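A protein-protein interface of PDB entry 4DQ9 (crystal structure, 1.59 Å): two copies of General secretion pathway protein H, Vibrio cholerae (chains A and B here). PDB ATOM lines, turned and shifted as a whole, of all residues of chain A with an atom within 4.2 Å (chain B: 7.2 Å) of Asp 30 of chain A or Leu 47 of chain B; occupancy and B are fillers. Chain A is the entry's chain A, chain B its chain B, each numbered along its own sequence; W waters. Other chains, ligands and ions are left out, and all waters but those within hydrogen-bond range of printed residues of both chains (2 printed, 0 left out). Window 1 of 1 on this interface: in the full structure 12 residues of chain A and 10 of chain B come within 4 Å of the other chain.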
ATOM      1  N   GLN A  29       2.129  11.005  19.964  1.00  0.00           N
ATOM      2  CA  GLN A  29       1.503  10.526  18.736  1.00  0.00           C
ATOM      3  C   GLN A  29       0.899   9.142  19.028  1.00  0.00           C
ATOM      4  O   GLN A  29       1.259   8.506  20.023  1.00  0.00           O
ATOM      5  CB  GLN A  29       2.451  10.478  17.545  1.00  0.00           C
ATOM      6  CG  GLN A  29       3.106  11.866  17.133  1.00  0.00           C
ATOM      7  CD  GLN A  29       2.163  13.126  16.819  1.00  0.00           C
ATOM      8  OE1 GLN A  29       1.183  13.073  16.032  1.00  0.00           O
ATOM      9  NE2 GLN A  29       2.537  14.276  17.403  1.00  0.00           N
ATOM     10  N   ASP A  30      -0.069   8.719  18.206  1.00  0.00           N
ATOM     11  CA  ASP A  30      -0.752   7.422  18.422  1.00  0.00           C
ATOM     12  C   ASP A  30      -0.185   6.418  17.407  1.00  0.00           C
ATOM     13  O   ASP A  30       0.121   6.736  16.219  1.00  0.00           O
ATOM     14  CB  ASP A  30      -2.233   7.484  18.176  1.00  0.00           C
ATOM     15  CG  ASP A  30      -3.027   8.260  19.206  1.00  0.00           C
ATOM     16  OD1 ASP A  30      -2.581   8.576  20.312  1.00  0.00           O
ATOM     17  OD2 ASP A  30      -4.194   8.561  18.861  1.00  0.00           O
ATOM     18  N   PHE A  31      -0.015   5.191  17.878  1.00  0.00           N
ATOM     19  CA  PHE A  31       0.443   4.043  17.105  1.00  0.00           C
ATOM     20  C   PHE A  31      -0.538   2.899  17.207  1.00  0.00           C
ATOM     21  O   PHE A  31      -1.552   3.040  17.854  1.00  0.00           O
ATOM     22  CB  PHE A  31       1.852   3.648  17.610  1.00  0.00           C
ATOM     23  CG  PHE A  31       2.874   4.731  17.393  1.00  0.00           C
ATOM     24  CD1 PHE A  31       3.081   5.753  18.347  1.00  0.00           C
ATOM     25  CD2 PHE A  31       3.637   4.792  16.224  1.00  0.00           C
ATOM     26  CE1 PHE A  31       3.998   6.743  18.155  1.00  0.00           C
ATOM     27  CE2 PHE A  31       4.530   5.817  16.019  1.00  0.00           C
ATOM     28  CZ  PHE A  31       4.750   6.773  16.957  1.00  0.00           C
ATOM     29  N   GLN A  46       1.477   4.047  12.535  1.00  0.00           N
ATOM     30  CA  GLN A  46       1.342   5.344  13.100  1.00  0.00           C
ATOM     31  C   GLN A  46       0.144   6.055  12.490  1.00  0.00           C
ATOM     32  O   GLN A  46      -0.126   5.927  11.330  1.00  0.00           O
ATOM     33  CB  GLN A  46       2.575   6.164  12.877  1.00  0.00           C
ATOM     34  CG  GLN A  46       2.583   7.548  13.592  1.00  0.00           C
ATOM     35  CD  GLN A  46       3.793   8.428  13.283  1.00  0.00           C
ATOM     36  OE1 GLN A  46       4.382   8.339  12.197  1.00  0.00           O
ATOM     37  NE2 GLN A  46       4.137   9.351  14.252  1.00  0.00           N
ATOM     38  N   LEU A  47      -0.595   6.761  13.327  1.00  0.00           N
ATOM     39  CA  LEU A  47      -1.735   7.545  12.825  1.00  0.00           C
ATOM     40  C   LEU A  47      -1.255   9.023  12.519  1.00  0.00           C
ATOM     41  O   LEU A  47      -0.593   9.699  13.381  1.00  0.00           O
ATOM     42  CB  LEU A  47      -2.799   7.579  13.915  1.00  0.00           C
ATOM     43  CG  LEU A  47      -4.021   8.416  13.538  1.00  0.00           C
ATOM     44  CD1 LEU A  47      -4.633   7.914  12.286  1.00  0.00           C
ATOM     45  CD2 LEU A  47      -5.044   8.438  14.693  1.00  0.00           C
ATOM     46  N   PHE A 116      -4.859  -0.366  19.444  1.00  0.00           N
ATOM     47  CA  PHE A 116      -4.466   0.988  19.549  1.00  0.00           C
ATOM     48  C   PHE A 116      -3.474   1.190  20.651  1.00  0.00           C
ATOM     49  O   PHE A 116      -3.635   0.650  21.769  1.00  0.00           O
ATOM     50  CB  PHE A 116      -5.669   1.926  19.690  1.00  0.00           C
ATOM     51  CG  PHE A 116      -6.709   1.719  18.630  1.00  0.00           C
ATOM     52  CD1 PHE A 116      -6.501   2.279  17.356  1.00  0.00           C
ATOM     53  CD2 PHE A 116      -7.872   1.035  18.860  1.00  0.00           C
ATOM     54  CE1 PHE A 116      -7.495   2.103  16.370  1.00  0.00           C
ATOM     55  CE2 PHE A 116      -8.815   0.777  17.789  1.00  0.00           C
ATOM     56  CZ  PHE A 116      -8.600   1.403  16.564  1.00  0.00           C
ATOM     57  N   VAL A 117      -2.474   1.996  20.356  1.00  0.00           N
ATOM     58  CA  VAL A 117      -1.364   2.275  21.269  1.00  0.00           C
ATOM     59  C   VAL A 117      -1.318   3.799  21.342  1.00  0.00           C
ATOM     60  O   VAL A 117      -0.588   4.444  20.562  1.00  0.00           O
ATOM     61  CB  VAL A 117      -0.068   1.630  20.823  1.00  0.00           C
ATOM     62  CG1 VAL A 117       1.152   1.949  21.834  1.00  0.00           C
ATOM     63  CG2 VAL A 117      -0.250   0.120  20.633  1.00  0.00           C
ATOM     64  N   LEU A 118      -2.138   4.329  22.251  1.00  0.00           N
ATOM     65  CA  LEU A 118      -2.429   5.753  22.244  1.00  0.00           C
ATOM     66  C   LEU A 118      -1.372   6.588  23.067  1.00  0.00           C
ATOM     67  O   LEU A 118      -0.706   6.085  23.972  1.00  0.00           O
ATOM     68  CB  LEU A 118      -3.793   6.015  22.793  1.00  0.00           C
ATOM     69  CG  LEU A 118      -4.991   5.238  22.192  1.00  0.00           C
ATOM     70  CD1 LEU A 118      -6.303   5.593  22.835  1.00  0.00           C
ATOM     71  CD2 LEU A 118      -4.981   5.426  20.730  1.00  0.00           C
ATOM     72  N   SER A 119      -1.312   7.884  22.754  1.00  0.00           N
ATOM     73  CA  SER A 119      -0.437   8.829  23.404  1.00  0.00           C
ATOM     74  C   SER A 119      -0.637   8.955  24.904  1.00  0.00           C
ATOM     75  O   SER A 119       0.287   9.331  25.634  1.00  0.00           O
ATOM     76  CB  SER A 119      -0.459  10.215  22.767  1.00  0.00           C
ATOM     77  OG  SER A 119      -1.771  10.683  22.872  1.00  0.00           O
ATOM     78  N   GLY B  28      -5.856  16.059  25.327  1.00  0.00           N
ATOM     79  CA  GLY B  28      -4.979  14.989  24.931  1.00  0.00           C
ATOM     80  C   GLY B  28      -5.630  13.769  24.316  1.00  0.00           C
ATOM     81  O   GLY B  28      -4.987  12.706  24.222  1.00  0.00           O
ATOM     82  N   GLN B  29      -6.946  13.805  23.987  1.00  0.00           N
ATOM     83  CA  GLN B  29      -7.587  12.719  23.336  1.00  0.00           C
ATOM     84  C   GLN B  29      -7.757  12.997  21.822  1.00  0.00           C
ATOM     85  O   GLN B  29      -7.731  14.156  21.384  1.00  0.00           O
ATOM     86  CB  GLN B  29      -8.955  12.397  23.964  1.00  0.00           C
ATOM     87  CG  GLN B  29      -8.923  12.221  25.466  1.00  0.00           C
ATOM     88  CD  GLN B  29      -8.217  10.977  25.959  1.00  0.00           C
ATOM     89  OE1 GLN B  29      -8.122   9.996  25.248  1.00  0.00           O
ATOM     90  NE2 GLN B  29      -7.706  11.017  27.198  1.00  0.00           N
ATOM     91  N   ASP B  30      -7.977  11.924  21.053  1.00  0.00           N
ATOM     92  CA  ASP B  30      -8.188  12.048  19.631  1.00  0.00           C
ATOM     93  C   ASP B  30      -9.664  11.950  19.322  1.00  0.00           C
ATOM     94  O   ASP B  30     -10.425  11.130  19.866  1.00  0.00           O
ATOM     95  CB  ASP B  30      -7.483  10.955  18.829  1.00  0.00           C
ATOM     96  CG  ASP B  30      -5.981  11.172  18.628  1.00  0.00           C
ATOM     97  OD1 ASP B  30      -5.358  12.175  19.092  1.00  0.00           O
ATOM     98  OD2 ASP B  30      -5.391  10.299  17.882  1.00  0.00           O
ATOM     99  N   PHE B  31     -10.014  12.756  18.319  1.00  0.00           N
ATOM    100  CA  PHE B  31     -11.352  12.772  17.809  1.00  0.00           C
ATOM    101  C   PHE B  31     -11.325  12.631  16.283  1.00  0.00           C
ATOM    102  O   PHE B  31     -10.294  12.539  15.640  1.00  0.00           O
ATOM    103  CB  PHE B  31     -12.022  14.066  18.262  1.00  0.00           C
ATOM    104  CG  PHE B  31     -12.214  14.171  19.745  1.00  0.00           C
ATOM    105  CD1 PHE B  31     -11.176  14.693  20.503  1.00  0.00           C
ATOM    106  CD2 PHE B  31     -13.387  13.731  20.390  1.00  0.00           C
ATOM    107  CE1 PHE B  31     -11.265  14.789  21.864  1.00  0.00           C
ATOM    108  CE2 PHE B  31     -13.503  13.866  21.784  1.00  0.00           C
ATOM    109  CZ  PHE B  31     -12.436  14.432  22.488  1.00  0.00           C
ATOM    110  N   GLY B  32     -12.530  12.642  15.704  1.00  0.00           N
ATOM    111  CA  GLY B  32     -12.621  12.526  14.227  1.00  0.00           C
ATOM    112  C   GLY B  32     -14.039  12.820  13.766  1.00  0.00           C
ATOM    113  O   GLY B  32     -14.981  12.862  14.565  1.00  0.00           O
ATOM    114  N   LEU B  45     -16.776  11.621  16.469  1.00  0.00           N
ATOM    115  CA  LEU B  45     -16.270  10.425  17.151  1.00  0.00           C
ATOM    116  C   LEU B  45     -15.108  10.727  18.032  1.00  0.00           C
ATOM    117  O   LEU B  45     -14.314  11.658  17.779  1.00  0.00           O
ATOM    118  CB  LEU B  45     -15.775   9.467  16.095  1.00  0.00           C
ATOM    119  CG  LEU B  45     -16.864   9.026  15.061  1.00  0.00           C
ATOM    120  CD1 LEU B  45     -16.281   8.190  13.844  1.00  0.00           C
ATOM    121  CD2 LEU B  45     -17.946   8.251  15.732  1.00  0.00           C
ATOM    122  N   GLN B  46     -14.859   9.826  18.984  1.00  0.00           N
ATOM    123  CA  GLN B  46     -13.704   9.870  19.872  1.00  0.00           C
ATOM    124  C   GLN B  46     -12.987   8.491  19.719  1.00  0.00           C
ATOM    125  O   GLN B  46     -13.712   7.511  19.579  1.00  0.00           O
ATOM    126  CB  GLN B  46     -14.142  10.078  21.338  1.00  0.00           C
ATOM    127  CG  GLN B  46     -13.038   9.976  22.238  1.00  0.00           C
ATOM    128  CD  GLN B  46     -13.465   9.904  23.726  1.00  0.00           C
ATOM    129  OE1 GLN B  46     -14.665   9.868  24.067  1.00  0.00           O
ATOM    130  NE2 GLN B  46     -12.448   9.844  24.598  1.00  0.00           N
ATOM    131  N   LEU B  47     -11.652   8.499  19.783  1.00  0.00           N
ATOM    132  CA  LEU B  47     -10.851   7.250  19.714  1.00  0.00           C
ATOM    133  C   LEU B  47     -10.574   6.810  21.145  1.00  0.00           C
ATOM    134  O   LEU B  47      -9.974   7.563  21.891  1.00  0.00           O
ATOM    135  CB  LEU B  47      -9.580   7.403  18.926  1.00  0.00           C
ATOM    136  CG  LEU B  47      -8.698   6.174  18.756  1.00  0.00           C
ATOM    137  CD1 LEU B  47      -9.502   4.991  18.155  1.00  0.00           C
ATOM    138  CD2 LEU B  47      -7.421   6.525  17.905  1.00  0.00           C
ATOM    139  N   THR B  48     -11.011   5.626  21.513  1.00  0.00           N
ATOM    140  CA  THR B  48     -10.597   5.058  22.771  1.00  0.00           C
ATOM    141  C   THR B  48      -9.926   3.722  22.464  1.00  0.00           C
ATOM    142  O   THR B  48     -10.180   3.076  21.449  1.00  0.00           O
ATOM    143  CB  THR B  48     -11.756   4.737  23.739  1.00  0.00           C
ATOM    144  OG1 THR B  48     -12.608   3.823  23.042  1.00  0.00           O
ATOM    145  CG2 THR B  48     -12.547   6.029  24.070  1.00  0.00           C
ATOM    146  N   ALA B  49      -9.046   3.344  23.383  1.00  0.00           N
ATOM    147  CA  ALA B  49      -8.254   2.131  23.216  1.00  0.00           C
ATOM    148  C   ALA B  49      -9.105   0.935  23.314  1.00  0.00           C
ATOM    149  O   ALA B  49      -8.944  -0.086  22.581  1.00  0.00           O
ATOM    150  CB  ALA B  49      -7.135   2.129  24.281  1.00  0.00           C
ATOM    151  N   ASP B  50     -10.019   0.997  24.286  1.00  0.00           N
ATOM    152  CA  ASP B  50     -10.782  -0.160  24.580  1.00  0.00           C
ATOM    153  C   ASP B  50     -11.944  -0.385  23.625  1.00  0.00           C
ATOM    154  O   ASP B  50     -12.337  -1.524  23.414  1.00  0.00           O
ATOM    155  CB  ASP B  50     -11.150  -0.206  26.111  1.00  0.00           C
ATOM    156  CG  ASP B  50     -11.803   1.084  26.603  1.00  0.00           C
ATOM    157  OD1 ASP B  50     -11.309   2.222  26.229  1.00  0.00           O
ATOM    158  OD2 ASP B  50     -12.839   0.964  27.349  1.00  0.00           O
ATOM    159  N   LYS B  51     -12.534   0.665  23.052  1.00  0.00           N
ATOM    160  CA  LYS B  51     -13.664   0.466  22.097  1.00  0.00           C
ATOM    161  C   LYS B  51     -13.451   1.038  20.670  1.00  0.00           C
ATOM    162  O   LYS B  51     -14.396   1.015  19.854  1.00  0.00           O
ATOM    163  CB  LYS B  51     -14.975   1.052  22.653  1.00  0.00           C
ATOM    164  CG  LYS B  51     -15.609   0.150  23.723  1.00  0.00           C
ATOM    165  CD  LYS B  51     -17.134   0.379  23.908  1.00  0.00           C
ATOM    166  CE  LYS B  51     -18.064  -0.278  22.816  1.00  0.00           C
ATOM    167  NZ  LYS B  51     -18.099  -1.775  22.755  1.00  0.00           N
ATOM    168  N   GLY B  52     -12.268   1.559  20.397  1.00  0.00           N
ATOM    169  CA  GLY B  52     -11.984   2.124  19.103  1.00  0.00           C
ATOM    170  C   GLY B  52     -12.791   3.392  18.924  1.00  0.00           C
ATOM    171  O   GLY B  52     -13.006   4.126  19.875  1.00  0.00           O
ATOM    172  N   TRP B  53     -13.188   3.657  17.696  1.00  0.00           N
ATOM    173  CA  TRP B  53     -13.892   4.913  17.426  1.00  0.00           C
ATOM    174  C   TRP B  53     -15.348   4.683  17.911  1.00  0.00           C
ATOM    175  O   TRP B  53     -15.992   3.640  17.602  1.00  0.00           O
ATOM    176  CB  TRP B  53     -13.887   5.223  15.924  1.00  0.00           C
ATOM    177  CG  TRP B  53     -12.590   5.650  15.403  1.00  0.00           C
ATOM    178  CD1 TRP B  53     -11.720   4.886  14.616  1.00  0.00           C
ATOM    179  CD2 TRP B  53     -11.941   6.904  15.598  1.00  0.00           C
ATOM    180  NE1 TRP B  53     -10.627   5.591  14.333  1.00  0.00           N
ATOM    181  CE2 TRP B  53     -10.708   6.832  14.934  1.00  0.00           C
ATOM    182  CE3 TRP B  53     -12.297   8.132  16.263  1.00  0.00           C
ATOM    183  CZ2 TRP B  53      -9.840   7.910  14.921  1.00  0.00           C
ATOM    184  CZ3 TRP B  53     -11.473   9.146  16.237  1.00  0.00           C
ATOM    185  CH2 TRP B  53     -10.249   9.055  15.556  1.00  0.00           C
ATOM    186  N   GLN B  54     -15.829   5.671  18.637  1.00  0.00           N
ATOM    187  CA  GLN B  54     -17.186   5.668  19.098  1.00  0.00           C
ATOM    188  C   GLN B  54     -17.749   7.072  19.081  1.00  0.00           C
ATOM    189  O   GLN B  54     -16.992   8.063  19.158  1.00  0.00           O
ATOM    190  CB  GLN B  54     -17.263   5.130  20.533  1.00  0.00           C
ATOM    191  CG  GLN B  54     -16.827   3.681  20.700  1.00  0.00           C
ATOM    192  CD  GLN B  54     -17.715   2.655  19.949  1.00  0.00           C
ATOM    193  OE1 GLN B  54     -18.894   2.891  19.641  1.00  0.00           O
ATOM    194  NE2 GLN B  54     -17.132   1.514  19.639  1.00  0.00           N
ATOM    195  N   PHE B 116      -9.510  13.139  10.697  1.00  0.00           N
ATOM    196  CA  PHE B 116      -8.864  12.956  12.009  1.00  0.00           C
ATOM    197  C   PHE B 116      -8.635  14.336  12.661  1.00  0.00           C
ATOM    198  O   PHE B 116      -8.187  15.276  11.987  1.00  0.00           O
ATOM    199  CB  PHE B 116      -7.554  12.216  11.838  1.00  0.00           C
ATOM    200  CG  PHE B 116      -7.733  10.811  11.240  1.00  0.00           C
ATOM    201  CD1 PHE B 116      -8.311   9.784  12.024  1.00  0.00           C
ATOM    202  CD2 PHE B 116      -7.414  10.550   9.932  1.00  0.00           C
ATOM    203  CE1 PHE B 116      -8.567   8.580  11.494  1.00  0.00           C
ATOM    204  CE2 PHE B 116      -7.597   9.282   9.411  1.00  0.00           C
ATOM    205  CZ  PHE B 116      -8.190   8.310  10.180  1.00  0.00           C
ATOM    206  N   LEU B 118      -6.686  15.321  15.766  1.00  0.00           N
ATOM    207  CA  LEU B 118      -5.801  14.664  16.691  1.00  0.00           C
ATOM    208  C   LEU B 118      -5.447  15.595  17.877  1.00  0.00           C
ATOM    209  O   LEU B 118      -5.476  16.842  17.781  1.00  0.00           O
ATOM    210  CB  LEU B 118      -4.532  14.243  15.955  1.00  0.00           C
ATOM    211  CG  LEU B 118      -4.826  13.306  14.746  1.00  0.00           C
ATOM    212  CD1 LEU B 118      -3.572  12.929  14.142  1.00  0.00           C
ATOM    213  CD2 LEU B 118      -5.704  12.109  15.140  1.00  0.00           C
ATOM    214  N   SER B 119      -5.014  14.969  18.949  1.00  0.00           N
ATOM    215  CA  SER B 119      -4.590  15.706  20.172  1.00  0.00           C
ATOM    216  C   SER B 119      -3.425  16.700  19.929  1.00  0.00           C
ATOM    217  O   SER B 119      -3.285  17.622  20.691  1.00  0.00           O
ATOM    218  CB  SER B 119      -4.259  14.725  21.261  1.00  0.00           C
ATOM    219  OG  SER B 119      -3.190  13.897  20.778  1.00  0.00           O
HETATM  220  O   HOH W   1      -2.555  12.245  24.925  1.00  0.00           O
HETATM  221  O   HOH W   2      -3.259  11.287  20.773  1.00  0.00           O
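Of the printed residues of chain B, Asp 30 of chain A touches Asp 30 (2.3 Å) and Leu 47 (3.9 Å). Of the printed residues of chain B, Leu 118 of chain A touches Leu 47 (3.9 Å) and Ala 49 (3.6 Å). Gly 28 of chain B touches none of the printed residues of chain A. Leu 47 of chain B touches three residues of chain A. Of the printed residues of chain A, Leu 118 of chain B touches Leu 47. The nearest printed residue of chain B that does not touch Asp 30 of chain A is Leu 118 of chain B (5.4 Å). The nearest printed residue of chain A that does not touch Leu 47 of chain B is Leu 47 of chain A (4.4 Å). The nearest printed residue of chain B that does not touch Phe 116 of chain A is Thr 48 of chain B (4.02 Å).
Among the printed residues, merely in contact across the chains: Asp 30 of chain A with Leu 47 of chain B (3.9 Å), Leu 47 of chain A with Asp 30 of chain B (3.7 Å), Leu 47 of chain A with Leu 118 of chain B (3.8 Å), Phe 116 of chain A with Leu 47 of chain B (3.9 Å), Phe 116 of chain A with Gly 52 of chain B (3.7 Å), Leu 118 of chain A with Leu 47 of chain B (3.9 Å) and Leu 118 of chain A with Ala 49 of chain B (3.6 Å).
O of Asp 30 of chain A lies within hydrogen-bond range of N of Leu 47 of chain A (3.0 Å). The backbone carbonyl oxygen (O) of Asp 30 of chain B lies within hydrogen-bond range of the backbone NH (N) of Leu 47 of chain B, 2.9 Å away. O of Gly 52 of chain B is in hydrogen-bond range of OG1 of Thr 48 of chain B. OD1 of Asp 30 of chain A is in hydrogen-bond range of N of Ser 119 of chain A (2.8 Å). The side-chain carboxylate of Asp 30 of chain B is in hydrogen-bond range of the backbone NH of Ser 119 of chain B (2.8 Å).
Asp 30 of chain A touches its own counterpart, Asp 30 of chain B. Asp 30 of chain A touches Leu 47 of chain B, and with the chains exchanged Leu 47 of chain A touches Asp 30 of chain B. Leu 47 of chain A touches Leu 118 of chain B, and with the chains exchanged Leu 118 of chain A touches Leu 47 of chain B. Phe 116 of chain A touches Leu 47 of chain B, but with the chains exchanged Leu 47 of chain A does not touch Phe 116 of chain B (4.1 Å). Positions printed for both chains: 29, 30, 31, 46, 47, 116, 118 and 119. Of the 8 pairs that touch across the chains among the printed residues, 5 have their exchanged pair printed and touching as well.
Water W1 bridges the backbone carbonyl oxygen (O) of Gly 28 of chain B (2.6 Å) and the side-chain hydroxyl (OG) of Ser 119 of chain A (2.7 Å). Water W2 lies within hydrogen-bond range of OG of Ser 119 of chain B (2.6 Å), OG of Ser 119 of chain A (2.6 Å), OD1 of Asp 30 of chain B (2.8 Å) and OD1 of Asp 30 of chain A (2.8 Å).
Of the 9 printed residues of chain A, 4 touch a printed residue of chain B. Hydrophobic or aromatic side chains of chain A that line the printed part of chain B: Leu 47, Phe 116 and Leu 118. Of the 18 printed residues of chain B, 5 touch a printed residue of chain A. Hydrophobic or aromatic side chains of chain B that line the printed part of chain A: Leu 47, Ala 49 and Leu 118.
The side-chain carboxylate (OD2) of Asp 30 of chain A sits close to the side-chain carboxylate (OD2) of Asp 30 of chain B, 2.3 Å away.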
